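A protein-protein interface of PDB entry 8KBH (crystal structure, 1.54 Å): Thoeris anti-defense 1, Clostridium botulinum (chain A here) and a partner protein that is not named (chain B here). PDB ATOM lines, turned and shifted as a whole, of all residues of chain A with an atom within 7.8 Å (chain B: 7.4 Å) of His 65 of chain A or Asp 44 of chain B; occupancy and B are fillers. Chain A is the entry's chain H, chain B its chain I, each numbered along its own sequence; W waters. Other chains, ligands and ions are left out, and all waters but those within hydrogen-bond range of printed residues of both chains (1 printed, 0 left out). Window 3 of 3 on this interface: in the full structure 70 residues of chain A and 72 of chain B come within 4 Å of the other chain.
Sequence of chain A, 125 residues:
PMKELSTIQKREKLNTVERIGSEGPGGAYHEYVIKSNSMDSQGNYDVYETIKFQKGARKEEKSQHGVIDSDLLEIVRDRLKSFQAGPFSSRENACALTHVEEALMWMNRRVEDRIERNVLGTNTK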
ATOM      1  N   LYS A  52      29.198 -37.317 -10.943  1.00  0.00           N
ATOM      2  CA  LYS A  52      30.224 -36.450 -11.511  1.00  0.00           C
ATOM      3  C   LYS A  52      30.082 -35.046 -10.934  1.00  0.00           C
ATOM      4  O   LYS A  52      28.979 -34.495 -10.894  1.00  0.00           O
ATOM      5  CB  LYS A  52      30.127 -36.393 -13.037  1.00  0.00           C
ATOM      6  CG  LYS A  52      30.175 -37.740 -13.727  1.00  0.00           C
ATOM      7  CD  LYS A  52      30.081 -37.575 -15.237  1.00  0.00           C
ATOM      8  CE  LYS A  52      30.605 -38.807 -15.947  1.00  0.00           C
ATOM      9  NZ  LYS A  52      29.702 -39.958 -15.706  1.00  0.00           N
ATOM     10  N   PHE A  53      31.196 -34.465 -10.511  1.00  0.00           N
ATOM     11  CA  PHE A  53      31.199 -33.156  -9.875  1.00  0.00           C
ATOM     12  C   PHE A  53      31.683 -32.081 -10.841  1.00  0.00           C
ATOM     13  O   PHE A  53      32.481 -32.347 -11.742  1.00  0.00           O
ATOM     14  CB  PHE A  53      32.093 -33.154  -8.634  1.00  0.00           C
ATOM     15  CG  PHE A  53      31.516 -33.894  -7.472  1.00  0.00           C
ATOM     16  CD1 PHE A  53      31.685 -35.270  -7.349  1.00  0.00           C
ATOM     17  CD2 PHE A  53      30.825 -33.216  -6.483  1.00  0.00           C
ATOM     18  CE1 PHE A  53      31.162 -35.961  -6.254  1.00  0.00           C
ATOM     19  CE2 PHE A  53      30.300 -33.897  -5.389  1.00  0.00           C
ATOM     20  CZ  PHE A  53      30.467 -35.272  -5.279  1.00  0.00           C
ATOM     21  N   GLN A  54      31.185 -30.862 -10.635  1.00  0.00           N
ATOM     22  CA  GLN A  54      31.711 -29.686 -11.321  1.00  0.00           C
ATOM     23  C   GLN A  54      33.226 -29.644 -11.218  1.00  0.00           C
ATOM     24  O   GLN A  54      33.796 -29.719 -10.124  1.00  0.00           O
ATOM     25  CB  GLN A  54      31.115 -28.412 -10.722  1.00  0.00           C
ATOM     26  CG  GLN A  54      31.474 -27.099 -11.444  1.00  0.00           C
ATOM     27  CD  GLN A  54      30.961 -27.047 -12.872  1.00  0.00           C
ATOM     28  OE1 GLN A  54      31.718 -26.848 -13.825  1.00  0.00           O
ATOM     29  NE2 GLN A  54      29.670 -27.291 -13.028  1.00  0.00           N
ATOM     30  N   LYS A  55      33.868 -29.518 -12.373  1.00  0.00           N
ATOM     31  CA  LYS A  55      35.320 -29.564 -12.486  1.00  0.00           C
ATOM     32  C   LYS A  55      35.719 -28.416 -13.401  1.00  0.00           C
ATOM     33  O   LYS A  55      35.494 -28.479 -14.613  1.00  0.00           O
ATOM     34  CB  LYS A  55      35.768 -30.919 -13.033  1.00  0.00           C
ATOM     35  CG  LYS A  55      37.255 -31.169 -13.042  1.00  0.00           C
ATOM     36  CD  LYS A  55      37.504 -32.664 -13.144  1.00  0.00           C
ATOM     37  CE  LYS A  55      38.555 -33.007 -14.180  1.00  0.00           C
ATOM     38  NZ  LYS A  55      38.646 -34.486 -14.336  1.00  0.00           N
ATOM     39  N   GLY A  56      36.277 -27.362 -12.822  1.00  0.00           N
ATOM     40  CA  GLY A  56      36.460 -26.115 -13.534  1.00  0.00           C
ATOM     41  C   GLY A  56      35.268 -25.186 -13.374  1.00  0.00           C
ATOM     42  O   GLY A  56      34.172 -25.583 -12.974  1.00  0.00           O
ATOM     43  N   ALA A  57      35.495 -23.917 -13.694  1.00  0.00           N
ATOM     44  CA  ALA A  57      34.441 -22.927 -13.551  1.00  0.00           C
ATOM     45  C   ALA A  57      33.252 -23.279 -14.436  1.00  0.00           C
ATOM     46  O   ALA A  57      33.413 -23.725 -15.576  1.00  0.00           O
ATOM     47  CB  ALA A  57      34.966 -21.532 -13.901  1.00  0.00           C
ATOM     48  N   ARG A  58      32.046 -23.080 -13.893  1.00  0.00           N
ATOM     49  CA  ARG A  58      30.815 -23.262 -14.658  1.00  0.00           C
ATOM     50  C   ARG A  58      30.765 -22.380 -15.907  1.00  0.00           C
ATOM     51  O   ARG A  58      29.951 -22.630 -16.805  1.00  0.00           O
ATOM     52  CB  ARG A  58      29.620 -22.996 -13.729  1.00  0.00           C
ATOM     53  CG  ARG A  58      28.217 -23.145 -14.329  1.00  0.00           C
ATOM     54  CD  ARG A  58      27.979 -24.486 -15.001  1.00  0.00           C
ATOM     55  NE  ARG A  58      27.774 -25.585 -14.060  1.00  0.00           N
ATOM     56  CZ  ARG A  58      26.713 -25.749 -13.273  1.00  0.00           C
ATOM     57  NH1 ARG A  58      25.705 -24.881 -13.285  1.00  0.00           N
ATOM     58  NH2 ARG A  58      26.660 -26.804 -12.466  1.00  0.00           N
ATOM     59  N   LYS A  59      31.642 -21.383 -16.009  1.00  0.00           N
ATOM     60  CA  LYS A  59      31.588 -20.431 -17.112  1.00  0.00           C
ATOM     61  C   LYS A  59      32.425 -20.830 -18.327  1.00  0.00           C
ATOM     62  O   LYS A  59      32.118 -20.389 -19.441  1.00  0.00           O
ATOM     63  CB  LYS A  59      31.997 -19.046 -16.609  1.00  0.00           C
ATOM     64  CG  LYS A  59      33.421 -18.953 -16.105  1.00  0.00           C
ATOM     65  CD  LYS A  59      33.689 -17.551 -15.574  1.00  0.00           C
ATOM     66  CE  LYS A  59      35.099 -17.404 -15.050  1.00  0.00           C
ATOM     67  NZ  LYS A  59      35.269 -18.237 -13.818  1.00  0.00           N
ATOM     68  N   GLU A  60      33.463 -21.645 -18.167  1.00  0.00           N
ATOM     69  CA  GLU A  60      34.163 -22.168 -19.334  1.00  0.00           C
ATOM     70  C   GLU A  60      33.377 -23.333 -19.926  1.00  0.00           C
ATOM     71  O   GLU A  60      32.773 -24.126 -19.200  1.00  0.00           O
ATOM     72  CB  GLU A  60      35.566 -22.658 -18.969  1.00  0.00           C
ATOM     73  CG  GLU A  60      36.350 -21.797 -17.989  1.00  0.00           C
ATOM     74  CD  GLU A  60      36.931 -20.543 -18.608  1.00  0.00           C
ATOM     75  OE1 GLU A  60      36.709 -20.299 -19.814  1.00  0.00           O
ATOM     76  OE2 GLU A  60      37.641 -19.810 -17.885  1.00  0.00           O
ATOM     77  N   GLU A  61      33.388 -23.441 -21.260  1.00  0.00           N
ATOM     78  CA  GLU A  61      32.896 -24.675 -21.867  1.00  0.00           C
ATOM     79  C   GLU A  61      33.889 -25.810 -21.678  1.00  0.00           C
ATOM     80  O   GLU A  61      33.509 -26.982 -21.771  1.00  0.00           O
ATOM     81  CB  GLU A  61      32.615 -24.492 -23.360  1.00  0.00           C
ATOM     82  CG  GLU A  61      33.855 -24.313 -24.222  1.00  0.00           C
ATOM     83  CD  GLU A  61      33.523 -24.152 -25.697  1.00  0.00           C
ATOM     84  OE1 GLU A  61      32.320 -24.134 -26.040  1.00  0.00           O
ATOM     85  OE2 GLU A  61      34.462 -24.063 -26.518  1.00  0.00           O
ATOM     86  N   LYS A  62      35.150 -25.468 -21.406  1.00  0.00           N
ATOM     87  CA  LYS A  62      36.190 -26.454 -21.137  1.00  0.00           C
ATOM     88  C   LYS A  62      35.777 -27.405 -20.021  1.00  0.00           C
ATOM     89  O   LYS A  62      36.102 -28.598 -20.051  1.00  0.00           O
ATOM     90  CB  LYS A  62      37.473 -25.715 -20.747  1.00  0.00           C
ATOM     91  CG  LYS A  62      37.992 -24.769 -21.815  1.00  0.00           C
ATOM     92  CD  LYS A  62      39.195 -23.982 -21.325  1.00  0.00           C
ATOM     93  CE  LYS A  62      39.653 -22.981 -22.379  1.00  0.00           C
ATOM     94  NZ  LYS A  62      40.830 -22.182 -21.936  1.00  0.00           N
ATOM     95  N   SER A  63      35.032 -26.893 -19.046  1.00  0.00           N
ATOM     96  CA  SER A  63      34.859 -27.543 -17.758  1.00  0.00           C
ATOM     97  C   SER A  63      33.989 -28.795 -17.856  1.00  0.00           C
ATOM     98  O   SER A  63      33.150 -28.944 -18.749  1.00  0.00           O
ATOM     99  CB  SER A  63      34.237 -26.560 -16.764  1.00  0.00           C
ATOM    100  OG  SER A  63      34.984 -25.354 -16.712  1.00  0.00           O
ATOM    101  N   GLN A  64      34.206 -29.703 -16.907  1.00  0.00           N
ATOM    102  CA  GLN A  64      33.317 -30.840 -16.674  1.00  0.00           C
ATOM    103  C   GLN A  64      32.195 -30.367 -15.758  1.00  0.00           C
ATOM    104  O   GLN A  64      32.359 -30.315 -14.536  1.00  0.00           O
ATOM    105  CB  GLN A  64      34.077 -32.003 -16.047  1.00  0.00           C
ATOM    106  CG  GLN A  64      33.199 -33.205 -15.705  1.00  0.00           C
ATOM    107  CD  GLN A  64      33.847 -34.155 -14.708  1.00  0.00           C
ATOM    108  OE1 GLN A  64      34.456 -35.157 -15.084  1.00  0.00           O
ATOM    109  NE2 GLN A  64      33.703 -33.847 -13.424  1.00  0.00           N
ATOM    110  N   HIS A  65      31.052 -30.011 -16.341  1.00  0.00           N
ATOM    111  CA  HIS A  65      29.941 -29.464 -15.569  1.00  0.00           C
ATOM    112  C   HIS A  65      29.230 -30.570 -14.798  1.00  0.00           C
ATOM    113  O   HIS A  65      28.892 -31.615 -15.362  1.00  0.00           O
ATOM    114  CB  HIS A  65      28.962 -28.741 -16.493  1.00  0.00           C
ATOM    115  CG  HIS A  65      29.604 -27.693 -17.347  1.00  0.00           C
ATOM    116  ND1 HIS A  65      30.500 -26.773 -16.846  1.00  0.00           N
ATOM    117  CD2 HIS A  65      29.479 -27.417 -18.667  1.00  0.00           C
ATOM    118  CE1 HIS A  65      30.904 -25.979 -17.822  1.00  0.00           C
ATOM    119  NE2 HIS A  65      30.296 -26.345 -18.936  1.00  0.00           N
ATOM    120  N   GLY A  66      29.007 -30.348 -13.512  1.00  0.00           N
ATOM    121  CA  GLY A  66      28.413 -31.373 -12.689  1.00  0.00           C
ATOM    122  C   GLY A  66      27.809 -30.829 -11.414  1.00  0.00           C
ATOM    123  O   GLY A  66      27.496 -29.643 -11.305  1.00  0.00           O
ATOM    124  N   VAL A  67      27.655 -31.723 -10.445  1.00  0.00           N
ATOM    125  CA  VAL A  67      27.050 -31.380  -9.172  1.00  0.00           C
ATOM    126  C   VAL A  67      28.120 -30.848  -8.228  1.00  0.00           C
ATOM    127  O   VAL A  67      29.325 -30.931  -8.490  1.00  0.00           O
ATOM    128  CB  VAL A  67      26.318 -32.592  -8.564  1.00  0.00           C
ATOM    129  CG1 VAL A  67      25.225 -33.063  -9.507  1.00  0.00           C
ATOM    130  CG2 VAL A  67      27.307 -33.713  -8.252  1.00  0.00           C
ATOM    131  N   ASN B  13      23.386 -25.130  -9.174  1.00  0.00           N
ATOM    132  CA  ASN B  13      22.346 -26.053  -9.596  1.00  0.00           C
ATOM    133  C   ASN B  13      21.126 -25.898  -8.699  1.00  0.00           C
ATOM    134  O   ASN B  13      21.181 -25.273  -7.633  1.00  0.00           O
ATOM    135  CB  ASN B  13      22.833 -27.510  -9.538  1.00  0.00           C
ATOM    136  CG  ASN B  13      24.179 -27.710 -10.205  1.00  0.00           C
ATOM    137  OD1 ASN B  13      24.404 -27.245 -11.319  1.00  0.00           O
ATOM    138  ND2 ASN B  13      25.075 -28.430  -9.538  1.00  0.00           N
ATOM    139  N   LYS B  33      19.777 -30.312 -11.372  1.00  0.00           N
ATOM    140  CA  LYS B  33      19.887 -29.782 -12.717  1.00  0.00           C
ATOM    141  C   LYS B  33      20.567 -28.428 -12.673  1.00  0.00           C
ATOM    142  O   LYS B  33      20.346 -27.631 -11.753  1.00  0.00           O
ATOM    143  CB  LYS B  33      18.523 -29.695 -13.406  1.00  0.00           C
ATOM    144  CG  LYS B  33      17.565 -28.678 -12.839  1.00  0.00           C
ATOM    145  CD  LYS B  33      16.147 -29.002 -13.288  1.00  0.00           C
ATOM    146  CE  LYS B  33      15.355 -27.743 -13.574  1.00  0.00           C
ATOM    147  NZ  LYS B  33      13.894 -27.986 -13.476  1.00  0.00           N
ATOM    148  N   SER B  34      21.419 -28.198 -13.666  1.00  0.00           N
ATOM    149  CA  SER B  34      22.190 -26.972 -13.724  1.00  0.00           C
ATOM    150  C   SER B  34      21.268 -25.776 -13.888  1.00  0.00           C
ATOM    151  O   SER B  34      20.170 -25.876 -14.443  1.00  0.00           O
ATOM    152  CB  SER B  34      23.195 -27.037 -14.875  1.00  0.00           C
ATOM    153  OG  SER B  34      22.536 -27.000 -16.133  1.00  0.00           O
ATOM    154  N   ASN B  35      21.714 -24.642 -13.351  1.00  0.00           N
ATOM    155  CA  ASN B  35      21.054 -23.372 -13.596  1.00  0.00           C
ATOM    156  C   ASN B  35      21.480 -22.779 -14.934  1.00  0.00           C
ATOM    157  O   ASN B  35      20.782 -21.914 -15.469  1.00  0.00           O
ATOM    158  CB  ASN B  35      21.372 -22.411 -12.453  1.00  0.00           C
ATOM    159  CG  ASN B  35      20.447 -22.592 -11.269  1.00  0.00           C
ATOM    160  OD1 ASN B  35      19.269 -22.893 -11.433  1.00  0.00           O
ATOM    161  ND2 ASN B  35      20.983 -22.433 -10.064  1.00  0.00           N
ATOM    162  N   SER B  36      22.605 -23.241 -15.473  1.00  0.00           N
ATOM    163  CA  SER B  36      23.112 -22.894 -16.792  1.00  0.00           C
ATOM    164  C   SER B  36      22.509 -23.809 -17.855  1.00  0.00           C
ATOM    165  O   SER B  36      21.989 -24.891 -17.562  1.00  0.00           O
ATOM    166  CB  SER B  36      24.638 -23.002 -16.816  1.00  0.00           C
ATOM    167  OG  SER B  36      25.052 -24.333 -17.099  1.00  0.00           O
ATOM    168  N   MET B  37      22.599 -23.372 -19.111  1.00  0.00           N
ATOM    169  CA  MET B  37      21.899 -24.052 -20.190  1.00  0.00           C
ATOM    170  C   MET B  37      22.803 -24.102 -21.416  1.00  0.00           C
ATOM    171  O   MET B  37      23.626 -23.207 -21.626  1.00  0.00           O
ATOM    172  CB  MET B  37      20.593 -23.320 -20.530  1.00  0.00           C
ATOM    173  CG  MET B  37      19.494 -23.605 -19.532  1.00  0.00           C
ATOM    174  SD  MET B  37      19.324 -25.350 -19.161  1.00  0.00           S
ATOM    175  CE  MET B  37      18.133 -25.869 -20.376  1.00  0.00           C
ATOM    176  N   ASP B  38      22.654 -25.150 -22.227  1.00  0.00           N
ATOM    177  CA  ASP B  38      23.392 -25.215 -23.480  1.00  0.00           C
ATOM    178  C   ASP B  38      22.577 -24.578 -24.609  1.00  0.00           C
ATOM    179  O   ASP B  38      21.475 -24.060 -24.402  1.00  0.00           O
ATOM    180  CB  ASP B  38      23.817 -26.655 -23.796  1.00  0.00           C
ATOM    181  CG  ASP B  38      22.654 -27.565 -24.189  1.00  0.00           C
ATOM    182  OD1 ASP B  38      21.513 -27.091 -24.379  1.00  0.00           O
ATOM    183  OD2 ASP B  38      22.890 -28.786 -24.309  1.00  0.00           O
ATOM    184  N   SER B  39      23.130 -24.623 -25.824  1.00  0.00           N
ATOM    185  CA  SER B  39      22.521 -23.923 -26.952  1.00  0.00           C
ATOM    186  C   SER B  39      21.105 -24.422 -27.226  1.00  0.00           C
ATOM    187  O   SER B  39      20.178 -23.623 -27.409  1.00  0.00           O
ATOM    188  CB  SER B  39      23.395 -24.083 -28.197  1.00  0.00           C
ATOM    189  OG  SER B  39      23.437 -25.438 -28.611  1.00  0.00           O
ATOM    190  N   GLN B  40      20.918 -25.738 -27.256  1.00  0.00           N
ATOM    191  CA  GLN B  40      19.644 -26.329 -27.650  1.00  0.00           C
ATOM    192  C   GLN B  40      18.594 -26.304 -26.544  1.00  0.00           C
ATOM    193  O   GLN B  40      17.515 -26.879 -26.730  1.00  0.00           O
ATOM    194  CB  GLN B  40      19.861 -27.770 -28.119  1.00  0.00           C
ATOM    195  CG  GLN B  40      20.976 -27.931 -29.142  1.00  0.00           C
ATOM    196  CD  GLN B  40      22.198 -28.634 -28.575  1.00  0.00           C
ATOM    197  OE1 GLN B  40      22.549 -28.454 -27.407  1.00  0.00           O
ATOM    198  NE2 GLN B  40      22.858 -29.436 -29.407  1.00  0.00           N
ATOM    199  N   GLY B  41      18.867 -25.659 -25.411  1.00  0.00           N
ATOM    200  CA  GLY B  41      17.916 -25.655 -24.318  1.00  0.00           C
ATOM    201  C   GLY B  41      17.891 -26.922 -23.496  1.00  0.00           C
ATOM    202  O   GLY B  41      16.870 -27.220 -22.866  1.00  0.00           O
ATOM    203  N   ASN B  42      18.978 -27.686 -23.495  1.00  0.00           N
ATOM    204  CA  ASN B  42      19.128 -28.854 -22.641  1.00  0.00           C
ATOM    205  C   ASN B  42      19.976 -28.473 -21.436  1.00  0.00           C
ATOM    206  O   ASN B  42      20.981 -27.768 -21.575  1.00  0.00           O
ATOM    207  CB  ASN B  42      19.787 -30.009 -23.401  1.00  0.00           C
ATOM    208  CG  ASN B  42      19.180 -30.226 -24.777  1.00  0.00           C
ATOM    209  OD1 ASN B  42      17.957 -30.215 -24.941  1.00  0.00           O
ATOM    210  ND2 ASN B  42      20.038 -30.410 -25.778  1.00  0.00           N
ATOM    211  N   TYR B  43      19.554 -28.910 -20.250  1.00  0.00           N
ATOM    212  CA  TYR B  43      20.341 -28.647 -19.053  1.00  0.00           C
ATOM    213  C   TYR B  43      21.770 -29.139 -19.236  1.00  0.00           C
ATOM    214  O   TYR B  43      22.008 -30.232 -19.761  1.00  0.00           O
ATOM    215  CB  TYR B  43      19.700 -29.307 -17.836  1.00  0.00           C
ATOM    216  CG  TYR B  43      18.296 -28.834 -17.536  1.00  0.00           C
ATOM    217  CD1 TYR B  43      18.045 -27.515 -17.182  1.00  0.00           C
ATOM    218  CD2 TYR B  43      17.233 -29.720 -17.534  1.00  0.00           C
ATOM    219  CE1 TYR B  43      16.762 -27.080 -16.895  1.00  0.00           C
ATOM    220  CE2 TYR B  43      15.946 -29.298 -17.236  1.00  0.00           C
ATOM    221  CZ  TYR B  43      15.718 -27.981 -16.921  1.00  0.00           C
ATOM    222  OH  TYR B  43      14.441 -27.571 -16.626  1.00  0.00           O
ATOM    223  N   ASP B  44      22.727 -28.301 -18.827  1.00  0.00           N
ATOM    224  CA  ASP B  44      24.128 -28.708 -18.864  1.00  0.00           C
ATOM    225  C   ASP B  44      24.417 -29.796 -17.839  1.00  0.00           C
ATOM    226  O   ASP B  44      25.330 -30.606 -18.036  1.00  0.00           O
ATOM    227  CB  ASP B  44      25.034 -27.500 -18.639  1.00  0.00           C
ATOM    228  CG  ASP B  44      25.188 -26.660 -19.887  1.00  0.00           C
ATOM    229  OD1 ASP B  44      24.242 -26.654 -20.700  1.00  0.00           O
ATOM    230  OD2 ASP B  44      26.251 -26.027 -20.065  1.00  0.00           O
ATOM    231  N   VAL B  45      23.662 -29.824 -16.743  1.00  0.00           N
ATOM    232  CA  VAL B  45      23.689 -30.916 -15.779  1.00  0.00           C
ATOM    233  C   VAL B  45      22.253 -31.355 -15.540  1.00  0.00           C
ATOM    234  O   VAL B  45      21.378 -30.516 -15.301  1.00  0.00           O
ATOM    235  CB  VAL B  45      24.366 -30.506 -14.456  1.00  0.00           C
ATOM    236  CG1 VAL B  45      24.373 -31.668 -13.471  1.00  0.00           C
ATOM    237  CG2 VAL B  45      25.788 -30.023 -14.717  1.00  0.00           C
ATOM    238  N   TYR B  46      22.002 -32.663 -15.655  1.00  0.00           N
ATOM    239  CA  TYR B  46      20.704 -33.229 -15.275  1.00  0.00           C
ATOM    240  C   TYR B  46      20.973 -34.647 -14.773  1.00  0.00           C
ATOM    241  O   TYR B  46      21.033 -35.594 -15.558  1.00  0.00           O
ATOM    242  CB  TYR B  46      19.707 -33.211 -16.428  1.00  0.00           C
ATOM    243  CG  TYR B  46      18.267 -33.358 -15.977  1.00  0.00           C
ATOM    244  CD1 TYR B  46      17.685 -34.606 -15.778  1.00  0.00           C
ATOM    245  CD2 TYR B  46      17.509 -32.234 -15.689  1.00  0.00           C
ATOM    246  CE1 TYR B  46      16.364 -34.720 -15.348  1.00  0.00           C
ATOM    247  CE2 TYR B  46      16.205 -32.332 -15.257  1.00  0.00           C
ATOM    248  CZ  TYR B  46      15.630 -33.569 -15.086  1.00  0.00           C
ATOM    249  OH  TYR B  46      14.325 -33.633 -14.646  1.00  0.00           O
ATOM    250  N   GLU B  47      21.133 -34.779 -13.458  1.00  0.00           N
ATOM    251  CA  GLU B  47      21.466 -36.056 -12.841  1.00  0.00           C
ATOM    252  C   GLU B  47      20.413 -36.453 -11.820  1.00  0.00           C
ATOM    253  O   GLU B  47      20.055 -35.660 -10.944  1.00  0.00           O
ATOM    254  CB  GLU B  47      22.849 -36.010 -12.194  1.00  0.00           C
ATOM    255  CG  GLU B  47      23.932 -36.474 -13.148  1.00  0.00           C
ATOM    256  CD  GLU B  47      23.641 -37.865 -13.699  1.00  0.00           C
ATOM    257  OE1 GLU B  47      23.715 -38.041 -14.937  1.00  0.00           O
ATOM    258  OE2 GLU B  47      23.343 -38.780 -12.895  1.00  0.00           O
HETATM  259  O   HOH W   1      25.078 -22.411 -13.723  1.00  0.00           O
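Of the 16 printed residues of chain A, 4 touch a printed residue of chain B.
Printed residues of chain A that touch a printed residue of chain B: Arg 58, His 65, Gly 66 and Val 67.
Hydrophobic or aromatic side chains of chain A that line the printed part of chain B: His 65.
Hydrophobic or aromatic side chains of chain B within 4 Å of the printed part of chain A: Val 45.
Among the printed residues, no Asp or Glu carboxylate lies within 4 Å of a Lys or Arg side-chain nitrogen of the other chain.
Water W1 bridges the guanidinium group of Arg 58 of chain A (2.6 Å) and the backbone NH of Ser 36 of chain B (3.1 Å).
NH1 of Arg 58 of chain A touches CB of Ser 34 of chain B (3.7 Å).
NH1 of Arg 58 of chain A touches N of Asn 35 of chain B, 3.999 Å away.
CD of Arg 58 of chain A touches OG of Ser 36 of chain B, at 3.6 Å.
His 65 of chain A touches Asp 44 of chain B.
His 65 of chain A touches Val 45 of chain B (C to CG2, 3.5 Å).
Gly 66 of chain A touches Val 45 of chain B.
Val 67 of chain A touches Asn 13 of chain B.
The guanidinium group (NH2) of Arg 58 of chain A sits at hydrogen-bond distance from the side-chain amide oxygen (OD1) of Asn 13 of chain B, 2.6 Å away.
The backbone carbonyl oxygen (O) of Gly 66 of chain A is in hydrogen-bond range of the side-chain amide nitrogen (ND2) of Asn 13 of chain B (3.2 Å).
The side-chain hydroxyl (OG) of Ser 34 of chain B lies within hydrogen-bond range of the backbone carbonyl oxygen (O) of Ser 36 of chain B (2.6 Å).
O of Val 45 of chain B sits at hydrogen-bond distance from N of Ser 34 of chain B (2.8 Å).
NE2 of Gln 54 of chain A lies close to N of Gly 66 of chain A (3.2 Å).
NH2 of Arg 58 of chain A sits at hydrogen-bond distance from O of Gly 66 of chain A (3.2 Å).
The backbone NH (N) of Asp 38 of chain B lies within hydrogen-bond range of the side-chain carboxylate (OD1) of Asp 44 of chain B, at 2.7 Å.
The backbone NH (N) of Val 67 of chain A sits at hydrogen-bond distance from the backbone carbonyl oxygen (O) of Lys 52 of chain A (3.1 Å).
His 65 of chain A touches two residues of chain B.
Of chain A, only His 65 comes within 4 Å of Asp 44 of chain B.
Of the printed residues of chain B, Arg 58 of chain A touches Asn 13 (2.6 Å), Ser 34 (3.7 Å), Asn 35 (3.999 Å) and Ser 36 (3.6 Å).
Printed residues of chain A within 4 Å of Val 45 of chain B: His 65 (3.5 Å) and Gly 66 (3.5 Å).
Of the printed residues of chain A, Asn 13 of chain B touches Arg 58 (2.6 Å), Gly 66 (3.2 Å) and Val 67 (3.6 Å).
Printed residues of chain B within 4 Å of Val 67 of chain A: Asn 13.
Printed residues of chain A within 4 Å of Asn 35 of chain B: Arg 58.
Asp 38 of chain B touches none of the printed residues of chain A.
Phe 53 of chain A touches none of the printed residues of chain B.
The nearest residue of chain B that does not touch His 65 of chain A is Ser 36 of chain B (5.6 Å).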
